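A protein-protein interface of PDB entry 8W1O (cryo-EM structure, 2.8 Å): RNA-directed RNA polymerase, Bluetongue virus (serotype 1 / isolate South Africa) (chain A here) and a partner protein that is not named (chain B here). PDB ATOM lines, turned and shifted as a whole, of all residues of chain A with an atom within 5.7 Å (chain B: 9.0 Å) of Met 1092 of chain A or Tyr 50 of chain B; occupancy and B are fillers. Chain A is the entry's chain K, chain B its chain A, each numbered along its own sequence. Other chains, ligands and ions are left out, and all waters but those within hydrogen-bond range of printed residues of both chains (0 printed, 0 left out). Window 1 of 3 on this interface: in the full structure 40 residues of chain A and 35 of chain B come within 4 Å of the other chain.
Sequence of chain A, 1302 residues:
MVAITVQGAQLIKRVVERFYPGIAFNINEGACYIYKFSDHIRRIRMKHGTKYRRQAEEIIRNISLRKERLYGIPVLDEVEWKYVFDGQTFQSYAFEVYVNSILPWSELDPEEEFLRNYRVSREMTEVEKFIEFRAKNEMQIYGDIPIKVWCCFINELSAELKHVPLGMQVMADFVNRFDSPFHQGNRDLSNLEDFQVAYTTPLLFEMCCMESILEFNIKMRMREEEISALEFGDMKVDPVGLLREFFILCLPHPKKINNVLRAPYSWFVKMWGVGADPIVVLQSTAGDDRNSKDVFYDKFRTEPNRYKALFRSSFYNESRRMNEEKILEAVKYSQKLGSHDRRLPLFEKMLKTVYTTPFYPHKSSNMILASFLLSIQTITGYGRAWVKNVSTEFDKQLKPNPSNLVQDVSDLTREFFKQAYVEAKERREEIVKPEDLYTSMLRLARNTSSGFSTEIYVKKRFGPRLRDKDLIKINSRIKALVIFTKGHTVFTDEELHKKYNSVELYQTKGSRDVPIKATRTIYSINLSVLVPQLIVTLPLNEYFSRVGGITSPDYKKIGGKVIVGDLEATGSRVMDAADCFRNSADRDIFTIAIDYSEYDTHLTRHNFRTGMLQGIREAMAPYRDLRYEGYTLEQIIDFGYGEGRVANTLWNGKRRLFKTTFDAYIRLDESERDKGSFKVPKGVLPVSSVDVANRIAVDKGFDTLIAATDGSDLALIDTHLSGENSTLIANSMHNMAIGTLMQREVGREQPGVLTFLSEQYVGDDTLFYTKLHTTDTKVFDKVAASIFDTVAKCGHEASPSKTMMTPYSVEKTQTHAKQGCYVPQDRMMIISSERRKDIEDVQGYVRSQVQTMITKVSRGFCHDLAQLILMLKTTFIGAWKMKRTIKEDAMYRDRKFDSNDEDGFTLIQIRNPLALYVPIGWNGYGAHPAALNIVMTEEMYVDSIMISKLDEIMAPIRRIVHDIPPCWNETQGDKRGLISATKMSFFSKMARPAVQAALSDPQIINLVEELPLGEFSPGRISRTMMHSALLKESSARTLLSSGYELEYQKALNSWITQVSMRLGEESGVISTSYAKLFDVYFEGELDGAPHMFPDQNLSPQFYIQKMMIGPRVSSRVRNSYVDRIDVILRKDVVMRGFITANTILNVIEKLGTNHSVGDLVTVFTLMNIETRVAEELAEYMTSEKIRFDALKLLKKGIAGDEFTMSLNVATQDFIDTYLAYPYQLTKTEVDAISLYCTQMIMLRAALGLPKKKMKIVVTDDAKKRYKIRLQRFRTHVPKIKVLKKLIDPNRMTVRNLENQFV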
ATOM      1  N   LEU A 282      -6.352  26.926   9.647  1.00  0.00           N
ATOM      2  CA  LEU A 282      -6.070  27.999  10.592  1.00  0.00           C
ATOM      3  C   LEU A 282      -7.079  29.116  10.357  1.00  0.00           C
ATOM      4  O   LEU A 282      -7.118  29.692   9.266  1.00  0.00           O
ATOM      5  CB  LEU A 282      -4.644  28.514  10.408  1.00  0.00           C
ATOM      6  CG  LEU A 282      -4.196  29.750  11.189  1.00  0.00           C
ATOM      7  CD1 LEU A 282      -4.143  29.472  12.680  1.00  0.00           C
ATOM      8  CD2 LEU A 282      -2.852  30.244  10.683  1.00  0.00           C
ATOM      9  N   TYR A 297      -5.090  36.186  12.907  1.00  0.00           N
ATOM     10  CA  TYR A 297      -5.199  34.739  13.029  1.00  0.00           C
ATOM     11  C   TYR A 297      -5.286  34.345  14.497  1.00  0.00           C
ATOM     12  O   TYR A 297      -4.656  34.966  15.357  1.00  0.00           O
ATOM     13  CB  TYR A 297      -3.998  34.041  12.376  1.00  0.00           C
ATOM     14  CG  TYR A 297      -3.598  34.624  11.038  1.00  0.00           C
ATOM     15  CD1 TYR A 297      -2.723  35.700  10.957  1.00  0.00           C
ATOM     16  CD2 TYR A 297      -4.090  34.093   9.855  1.00  0.00           C
ATOM     17  CE1 TYR A 297      -2.362  36.235   9.737  1.00  0.00           C
ATOM     18  CE2 TYR A 297      -3.730  34.620   8.630  1.00  0.00           C
ATOM     19  CZ  TYR A 297      -2.866  35.689   8.578  1.00  0.00           C
ATOM     20  OH  TYR A 297      -2.505  36.216   7.360  1.00  0.00           O
ATOM     21  N   ASP A 298      -6.074  33.304  14.786  1.00  0.00           N
ATOM     22  CA  ASP A 298      -6.260  32.954  16.193  1.00  0.00           C
ATOM     23  C   ASP A 298      -5.832  31.537  16.560  1.00  0.00           C
ATOM     24  O   ASP A 298      -5.093  31.374  17.534  1.00  0.00           O
ATOM     25  CB  ASP A 298      -7.724  33.183  16.603  1.00  0.00           C
ATOM     26  CG  ASP A 298      -8.696  32.466  15.708  1.00  0.00           C
ATOM     27  OD1 ASP A 298      -8.240  31.865  14.717  1.00  0.00           O
ATOM     28  OD2 ASP A 298      -9.909  32.501  15.995  1.00  0.00           O
ATOM     29  N   LYS A 299      -6.274  30.511  15.828  1.00  0.00           N
ATOM     30  CA  LYS A 299      -5.981  29.139  16.248  1.00  0.00           C
ATOM     31  C   LYS A 299      -6.305  28.157  15.127  1.00  0.00           C
ATOM     32  O   LYS A 299      -6.939  28.503  14.127  1.00  0.00           O
ATOM     33  CB  LYS A 299      -6.761  28.746  17.505  1.00  0.00           C
ATOM     34  CG  LYS A 299      -8.252  29.010  17.412  1.00  0.00           C
ATOM     35  CD  LYS A 299      -8.930  28.778  18.752  1.00  0.00           C
ATOM     36  CE  LYS A 299     -10.332  29.364  18.772  1.00  0.00           C
ATOM     37  NZ  LYS A 299     -11.286  28.555  17.966  1.00  0.00           N
ATOM     38  N   PHE A 300      -5.867  26.914  15.328  1.00  0.00           N
ATOM     39  CA  PHE A 300      -6.142  25.797  14.436  1.00  0.00           C
ATOM     40  C   PHE A 300      -7.425  25.078  14.842  1.00  0.00           C
ATOM     41  O   PHE A 300      -7.845  25.123  16.001  1.00  0.00           O
ATOM     42  CB  PHE A 300      -4.989  24.791  14.453  1.00  0.00           C
ATOM     43  CG  PHE A 300      -3.772  25.231  13.695  1.00  0.00           C
ATOM     44  CD1 PHE A 300      -3.745  25.176  12.312  1.00  0.00           C
ATOM     45  CD2 PHE A 300      -2.644  25.673  14.364  1.00  0.00           C
ATOM     46  CE1 PHE A 300      -2.624  25.571  11.612  1.00  0.00           C
ATOM     47  CE2 PHE A 300      -1.519  26.069  13.668  1.00  0.00           C
ATOM     48  CZ  PHE A 300      -1.510  26.017  12.292  1.00  0.00           C
ATOM     49  N   HIS A 362      -0.024  22.163  10.565  1.00  0.00           N
ATOM     50  CA  HIS A 362       0.536  22.322  11.899  1.00  0.00           C
ATOM     51  C   HIS A 362       1.660  21.340  12.196  1.00  0.00           C
ATOM     52  O   HIS A 362       2.246  21.402  13.281  1.00  0.00           O
ATOM     53  CB  HIS A 362      -0.568  22.172  12.950  1.00  0.00           C
ATOM     54  CG  HIS A 362      -1.182  20.808  12.992  1.00  0.00           C
ATOM     55  ND1 HIS A 362      -1.989  20.322  11.986  1.00  0.00           N
ATOM     56  CD2 HIS A 362      -1.107  19.825  13.921  1.00  0.00           C
ATOM     57  CE1 HIS A 362      -2.385  19.100  12.293  1.00  0.00           C
ATOM     58  NE2 HIS A 362      -1.863  18.775  13.461  1.00  0.00           N
ATOM     59  N   PRO A1090       1.618  33.207  23.589  1.00  0.00           N
ATOM     60  CA  PRO A1090       2.250  33.217  22.267  1.00  0.00           C
ATOM     61  C   PRO A1090       1.284  33.653  21.176  1.00  0.00           C
ATOM     62  O   PRO A1090       0.068  33.471  21.275  1.00  0.00           O
ATOM     63  CB  PRO A1090       2.689  31.763  22.072  1.00  0.00           C
ATOM     64  CG  PRO A1090       1.786  30.974  22.946  1.00  0.00           C
ATOM     65  CD  PRO A1090       1.465  31.843  24.124  1.00  0.00           C
ATOM     66  N   HIS A1091       1.847  34.233  20.121  1.00  0.00           N
ATOM     67  CA  HIS A1091       1.078  34.751  19.001  1.00  0.00           C
ATOM     68  C   HIS A1091       1.028  33.736  17.866  1.00  0.00           C
ATOM     69  O   HIS A1091       1.934  32.916  17.701  1.00  0.00           O
ATOM     70  CB  HIS A1091       1.674  36.065  18.494  1.00  0.00           C
ATOM     71  CG  HIS A1091       1.475  37.221  19.423  1.00  0.00           C
ATOM     72  ND1 HIS A1091       2.412  37.590  20.362  1.00  0.00           N
ATOM     73  CD2 HIS A1091       0.447  38.091  19.556  1.00  0.00           C
ATOM     74  CE1 HIS A1091       1.971  38.638  21.034  1.00  0.00           C
ATOM     75  NE2 HIS A1091       0.780  38.963  20.564  1.00  0.00           N
ATOM     76  N   MET A1092      -0.044  33.805  17.084  1.00  0.00           N
ATOM     77  CA  MET A1092      -0.246  32.929  15.938  1.00  0.00           C
ATOM     78  C   MET A1092       0.047  33.671  14.644  1.00  0.00           C
ATOM     79  O   MET A1092      -0.355  34.824  14.468  1.00  0.00           O
ATOM     80  CB  MET A1092      -1.671  32.382  15.914  1.00  0.00           C
ATOM     81  CG  MET A1092      -1.989  31.464  17.069  1.00  0.00           C
ATOM     82  SD  MET A1092      -0.922  30.015  17.070  1.00  0.00           S
ATOM     83  CE  MET A1092      -1.528  29.161  15.620  1.00  0.00           C
ATOM     84  N   PHE A1093       0.749  32.996  13.738  1.00  0.00           N
ATOM     85  CA  PHE A1093       1.161  33.563  12.464  1.00  0.00           C
ATOM     86  C   PHE A1093       0.994  32.496  11.394  1.00  0.00           C
ATOM     87  O   PHE A1093       1.109  31.302  11.693  1.00  0.00           O
ATOM     88  CB  PHE A1093       2.615  34.063  12.511  1.00  0.00           C
ATOM     89  CG  PHE A1093       3.575  33.103  13.159  1.00  0.00           C
ATOM     90  CD1 PHE A1093       3.737  33.078  14.536  1.00  0.00           C
ATOM     91  CD2 PHE A1093       4.327  32.237  12.388  1.00  0.00           C
ATOM     92  CE1 PHE A1093       4.620  32.200  15.126  1.00  0.00           C
ATOM     93  CE2 PHE A1093       5.212  31.358  12.974  1.00  0.00           C
ATOM     94  CZ  PHE A1093       5.360  31.341  14.344  1.00  0.00           C
ATOM     95  N   PRO A1094       0.721  32.887  10.144  1.00  0.00           N
ATOM     96  CA  PRO A1094       0.460  31.879   9.107  1.00  0.00           C
ATOM     97  C   PRO A1094       1.709  31.260   8.510  1.00  0.00           C
ATOM     98  O   PRO A1094       1.600  30.220   7.848  1.00  0.00           O
ATOM     99  CB  PRO A1094      -0.311  32.671   8.047  1.00  0.00           C
ATOM    100  CG  PRO A1094       0.247  34.042   8.162  1.00  0.00           C
ATOM    101  CD  PRO A1094       0.563  34.256   9.624  1.00  0.00           C
ATOM    102  N   GLN A1096       4.557  29.185   8.930  1.00  0.00           N
ATOM    103  CA  GLN A1096       5.327  28.156   9.615  1.00  0.00           C
ATOM    104  C   GLN A1096       6.577  27.861   8.787  1.00  0.00           C
ATOM    105  O   GLN A1096       6.921  28.588   7.850  1.00  0.00           O
ATOM    106  CB  GLN A1096       4.472  26.913   9.838  1.00  0.00           C
ATOM    107  CG  GLN A1096       3.072  27.192  10.371  1.00  0.00           C
ATOM    108  CD  GLN A1096       3.076  27.705  11.796  1.00  0.00           C
ATOM    109  OE1 GLN A1096       3.700  27.116  12.677  1.00  0.00           O
ATOM    110  NE2 GLN A1096       2.375  28.808  12.032  1.00  0.00           N
ATOM    111  N   TYR A1103      11.532  31.679  14.509  1.00  0.00           N
ATOM    112  CA  TYR A1103      10.273  31.224  15.086  1.00  0.00           C
ATOM    113  C   TYR A1103      10.052  31.815  16.472  1.00  0.00           C
ATOM    114  O   TYR A1103       8.931  32.204  16.814  1.00  0.00           O
ATOM    115  CB  TYR A1103      10.243  29.697  15.136  1.00  0.00           C
ATOM    116  CG  TYR A1103       8.854  29.100  15.122  1.00  0.00           C
ATOM    117  CD1 TYR A1103       8.089  29.041  16.278  1.00  0.00           C
ATOM    118  CD2 TYR A1103       8.311  28.588  13.952  1.00  0.00           C
ATOM    119  CE1 TYR A1103       6.822  28.494  16.269  1.00  0.00           C
ATOM    120  CE2 TYR A1103       7.044  28.038  13.933  1.00  0.00           C
ATOM    121  CZ  TYR A1103       6.305  27.994  15.095  1.00  0.00           C
ATOM    122  OH  TYR A1103       5.043  27.448  15.084  1.00  0.00           O
ATOM    123  N   PRO A1111       2.735  39.090  14.629  1.00  0.00           N
ATOM    124  CA  PRO A1111       2.773  39.654  13.279  1.00  0.00           C
ATOM    125  C   PRO A1111       2.221  41.072  13.258  1.00  0.00           C
ATOM    126  O   PRO A1111       1.415  41.469  14.100  1.00  0.00           O
ATOM    127  CB  PRO A1111       1.882  38.706  12.467  1.00  0.00           C
ATOM    128  CG  PRO A1111       1.684  37.500  13.339  1.00  0.00           C
ATOM    129  CD  PRO A1111       1.757  37.998  14.737  1.00  0.00           C
ATOM    130  N   LYS B  42      10.694  25.790  24.001  1.00  0.00           N
ATOM    131  CA  LYS B  42       9.489  26.597  23.825  1.00  0.00           C
ATOM    132  C   LYS B  42       8.798  26.278  22.504  1.00  0.00           C
ATOM    133  O   LYS B  42       7.562  26.195  22.441  1.00  0.00           O
ATOM    134  CB  LYS B  42       9.841  28.082  23.903  1.00  0.00           C
ATOM    135  CG  LYS B  42      10.432  28.511  25.233  1.00  0.00           C
ATOM    136  CD  LYS B  42      10.811  29.983  25.219  1.00  0.00           C
ATOM    137  CE  LYS B  42      11.404  30.414  26.550  1.00  0.00           C
ATOM    138  NZ  LYS B  42      11.837  31.837  26.532  1.00  0.00           N
ATOM    139  N   VAL B  43       9.581  26.101  21.438  1.00  0.00           N
ATOM    140  CA  VAL B  43       9.004  25.730  20.145  1.00  0.00           C
ATOM    141  C   VAL B  43       8.323  24.366  20.239  1.00  0.00           C
ATOM    142  O   VAL B  43       7.218  24.162  19.718  1.00  0.00           O
ATOM    143  CB  VAL B  43      10.081  25.754  19.045  1.00  0.00           C
ATOM    144  CG1 VAL B  43       9.508  25.268  17.726  1.00  0.00           C
ATOM    145  CG2 VAL B  43      10.641  27.155  18.887  1.00  0.00           C
ATOM    146  N   ARG B  44       8.969  23.414  20.918  1.00  0.00           N
ATOM    147  CA  ARG B  44       8.365  22.096  21.099  1.00  0.00           C
ATOM    148  C   ARG B  44       7.072  22.182  21.902  1.00  0.00           C
ATOM    149  O   ARG B  44       6.097  21.486  21.596  1.00  0.00           O
ATOM    150  CB  ARG B  44       9.353  21.151  21.783  1.00  0.00           C
ATOM    151  CG  ARG B  44      10.548  20.756  20.933  1.00  0.00           C
ATOM    152  CD  ARG B  44      10.131  20.075  19.639  1.00  0.00           C
ATOM    153  NE  ARG B  44      10.142  20.992  18.505  1.00  0.00           N
ATOM    154  CZ  ARG B  44      11.231  21.347  17.838  1.00  0.00           C
ATOM    155  NH1 ARG B  44      12.426  20.887  18.170  1.00  0.00           N
ATOM    156  NH2 ARG B  44      11.119  22.188  16.814  1.00  0.00           N
ATOM    157  N   GLN B  45       7.046  23.028  22.934  1.00  0.00           N
ATOM    158  CA  GLN B  45       5.844  23.171  23.750  1.00  0.00           C
ATOM    159  C   GLN B  45       4.691  23.757  22.945  1.00  0.00           C
ATOM    160  O   GLN B  45       3.551  23.289  23.046  1.00  0.00           O
ATOM    161  CB  GLN B  45       6.128  24.040  24.974  1.00  0.00           C
ATOM    162  CG  GLN B  45       7.040  23.404  26.004  1.00  0.00           C
ATOM    163  CD  GLN B  45       7.636  24.428  26.948  1.00  0.00           C
ATOM    164  OE1 GLN B  45       7.028  25.462  27.224  1.00  0.00           O
ATOM    165  NE2 GLN B  45       8.837  24.148  27.443  1.00  0.00           N
ATOM    166  N   VAL B  46       4.961  24.793  22.149  1.00  0.00           N
ATOM    167  CA  VAL B  46       3.872  25.398  21.385  1.00  0.00           C
ATOM    168  C   VAL B  46       3.395  24.443  20.291  1.00  0.00           C
ATOM    169  O   VAL B  46       2.199  24.386  19.978  1.00  0.00           O
ATOM    170  CB  VAL B  46       4.281  26.779  20.830  1.00  0.00           C
ATOM    171  CG1 VAL B  46       5.399  26.682  19.818  1.00  0.00           C
ATOM    172  CG2 VAL B  46       3.079  27.503  20.244  1.00  0.00           C
ATOM    173  N   GLN B  47       4.304  23.639  19.728  1.00  0.00           N
ATOM    174  CA  GLN B  47       3.881  22.631  18.760  1.00  0.00           C
ATOM    175  C   GLN B  47       3.034  21.543  19.418  1.00  0.00           C
ATOM    176  O   GLN B  47       2.055  21.065  18.829  1.00  0.00           O
ATOM    177  CB  GLN B  47       5.102  22.028  18.067  1.00  0.00           C
ATOM    178  CG  GLN B  47       5.712  22.943  17.019  1.00  0.00           C
ATOM    179  CD  GLN B  47       7.054  22.455  16.518  1.00  0.00           C
ATOM    180  OE1 GLN B  47       7.788  21.775  17.235  1.00  0.00           O
ATOM    181  NE2 GLN B  47       7.384  22.802  15.280  1.00  0.00           N
ATOM    182  N   ALA B  48       3.392  21.137  20.638  1.00  0.00           N
ATOM    183  CA  ALA B  48       2.578  20.161  21.358  1.00  0.00           C
ATOM    184  C   ALA B  48       1.204  20.728  21.690  1.00  0.00           C
ATOM    185  O   ALA B  48       0.198  20.009  21.651  1.00  0.00           O
ATOM    186  CB  ALA B  48       3.297  19.712  22.630  1.00  0.00           C
ATOM    187  N   ASP B  49       1.147  22.018  22.029  1.00  0.00           N
ATOM    188  CA  ASP B  49      -0.137  22.677  22.245  1.00  0.00           C
ATOM    189  C   ASP B  49      -0.965  22.698  20.967  1.00  0.00           C
ATOM    190  O   ASP B  49      -2.193  22.563  21.011  1.00  0.00           O
ATOM    191  CB  ASP B  49       0.081  24.095  22.771  1.00  0.00           C
ATOM    192  CG  ASP B  49       0.579  24.116  24.204  1.00  0.00           C
ATOM    193  OD1 ASP B  49       0.991  23.051  24.710  1.00  0.00           O
ATOM    194  OD2 ASP B  49       0.560  25.198  24.826  1.00  0.00           O
ATOM    195  N   TYR B  50      -0.309  22.878  19.816  1.00  0.00           N
ATOM    196  CA  TYR B  50      -1.010  22.752  18.540  1.00  0.00           C
ATOM    197  C   TYR B  50      -1.557  21.341  18.355  1.00  0.00           C
ATOM    198  O   TYR B  50      -2.673  21.159  17.858  1.00  0.00           O
ATOM    199  CB  TYR B  50      -0.077  23.104  17.378  1.00  0.00           C
ATOM    200  CG  TYR B  50       0.368  24.548  17.305  1.00  0.00           C
ATOM    201  CD1 TYR B  50      -0.146  25.508  18.166  1.00  0.00           C
ATOM    202  CD2 TYR B  50       1.321  24.945  16.377  1.00  0.00           C
ATOM    203  CE1 TYR B  50       0.270  26.821  18.098  1.00  0.00           C
ATOM    204  CE2 TYR B  50       1.743  26.253  16.304  1.00  0.00           C
ATOM    205  CZ  TYR B  50       1.215  27.187  17.165  1.00  0.00           C
ATOM    206  OH  TYR B  50       1.635  28.494  17.090  1.00  0.00           O
ATOM    207  N   MET B  51      -0.772  20.333  18.739  1.00  0.00           N
ATOM    208  CA  MET B  51      -1.202  18.945  18.582  1.00  0.00           C
ATOM    209  C   MET B  51      -2.380  18.608  19.491  1.00  0.00           C
ATOM    210  O   MET B  51      -3.227  17.782  19.129  1.00  0.00           O
ATOM    211  CB  MET B  51      -0.037  17.994  18.853  1.00  0.00           C
ATOM    212  CG  MET B  51       1.094  18.087  17.847  1.00  0.00           C
ATOM    213  SD  MET B  51       0.548  17.679  16.180  1.00  0.00           S
ATOM    214  CE  MET B  51       0.236  15.925  16.359  1.00  0.00           C
ATOM    215  N   THR B  52      -2.438  19.208  20.685  1.00  0.00           N
ATOM    216  CA  THR B  52      -3.557  18.935  21.585  1.00  0.00           C
ATOM    217  C   THR B  52      -4.875  19.405  20.985  1.00  0.00           C
ATOM    218  O   THR B  52      -5.889  18.701  21.062  1.00  0.00           O
ATOM    219  CB  THR B  52      -3.327  19.593  22.945  1.00  0.00           C
ATOM    220  OG1 THR B  52      -2.825  20.922  22.760  1.00  0.00           O
ATOM    221  CG2 THR B  52      -2.330  18.788  23.760  1.00  0.00           C
ATOM    222  N   ALA B  53      -4.884  20.590  20.382  1.00  0.00           N
ATOM    223  CA  ALA B  53      -6.022  21.004  19.580  1.00  0.00           C
ATOM    224  C   ALA B  53      -6.035  20.226  18.269  1.00  0.00           C
ATOM    225  O   ALA B  53      -5.066  19.550  17.912  1.00  0.00           O
ATOM    226  CB  ALA B  53      -5.981  22.507  19.311  1.00  0.00           C
ATOM    227  N   THR B  54      -7.157  20.320  17.553  1.00  0.00           N
ATOM    228  CA  THR B  54      -7.435  19.580  16.321  1.00  0.00           C
ATOM    229  C   THR B  54      -7.394  18.071  16.516  1.00  0.00           C
ATOM    230  O   THR B  54      -7.278  17.331  15.532  1.00  0.00           O
ATOM    231  CB  THR B  54      -6.482  19.957  15.175  1.00  0.00           C
ATOM    232  OG1 THR B  54      -5.209  19.333  15.380  1.00  0.00           O
ATOM    233  CG2 THR B  54      -6.298  21.460  15.093  1.00  0.00           C
ATOM    234  N   ARG B  55      -7.484  17.590  17.756  1.00  0.00           N
ATOM    235  CA  ARG B  55      -7.473  16.154  18.004  1.00  0.00           C
ATOM    236  C   ARG B  55      -8.788  15.494  17.614  1.00  0.00           C
ATOM    237  O   ARG B  55      -8.787  14.344  17.160  1.00  0.00           O
ATOM    238  CB  ARG B  55      -7.168  15.880  19.476  1.00  0.00           C
ATOM    239  CG  ARG B  55      -6.783  14.443  19.771  1.00  0.00           C
ATOM    240  CD  ARG B  55      -6.567  14.229  21.256  1.00  0.00           C
ATOM    241  NE  ARG B  55      -6.124  12.873  21.553  1.00  0.00           N
ATOM    242  CZ  ARG B  55      -6.935  11.831  21.671  1.00  0.00           C
ATOM    243  NH1 ARG B  55      -8.242  11.950  21.504  1.00  0.00           N
ATOM    244  NH2 ARG B  55      -6.423  10.639  21.961  1.00  0.00           N
ATOM    245  N   GLU B  56      -9.909  16.192  17.778  1.00  0.00           N
ATOM    246  CA  GLU B  56     -11.217  15.634  17.475  1.00  0.00           C
ATOM    247  C   GLU B  56     -12.003  16.610  16.610  1.00  0.00           C
ATOM    248  O   GLU B  56     -11.878  17.830  16.748  1.00  0.00           O
ATOM    249  CB  GLU B  56     -12.002  15.303  18.758  1.00  0.00           C
ATOM    250  CG  GLU B  56     -12.457  16.513  19.566  1.00  0.00           C
ATOM    251  CD  GLU B  56     -11.392  17.032  20.515  1.00  0.00           C
ATOM    252  OE1 GLU B  56     -10.209  16.666  20.355  1.00  0.00           O
ATOM    253  OE2 GLU B  56     -11.740  17.812  21.426  1.00  0.00           O
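OH of Tyr 1103 of chain A lies within hydrogen-bond range of OE1 of Gln 1096 of chain A (2.8 Å).
Of chain B, only Tyr 50 (3.0 Å) comes within 4 Å of Met 1092 of chain A.
Of chain A, only Met 1092 and Tyr 1103 come within 4 Å of Tyr 50 of chain B.
Printed residues of chain B within 4 Å of Tyr 1103 of chain A: Tyr 50.
Of the printed residues of chain B, His 362 of chain A touches Met 51 (3.5 Å) and Thr 54 (3.9 Å).
Of the printed residues of chain A, Thr 54 of chain B touches Phe 300 (3.6 Å) and His 362 (3.9 Å).
The nearest residue of chain B that does not touch Met 1092 of chain A is Val 46 of chain B (5.7 Å).
The nearest printed residue of chain A that does not touch Thr 54 of chain B is Lys 299 of chain A (6.7 Å).
Among the printed residues, pairs that only touch across the chains: Phe 300 of chain A with Thr 54 of chain B (3.6 Å), Tyr 1103 of chain A with Tyr 50 of chain B (3.7 Å) and His 362 of chain A with Thr 54 of chain B (3.9 Å).
The side-chain sulfur (SD) of Met 51 of chain B sits close to a ring nitrogen (NE2) of His 362 of chain A, 3.8 Å away.
The side-chain sulfur (SD) of Met 1092 of chain A is in hydrogen-bond range of the side-chain hydroxyl (OH) of Tyr 50 of chain B (3.0 Å).
Printed residues of chain A that touch a printed residue of chain B: Phe 300, His 362, Met 1092 and Tyr 1103.
Among the printed residues, no Asp or Glu carboxylate lies within 4 Å of a Lys or Arg side-chain nitrogen of the other chain.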
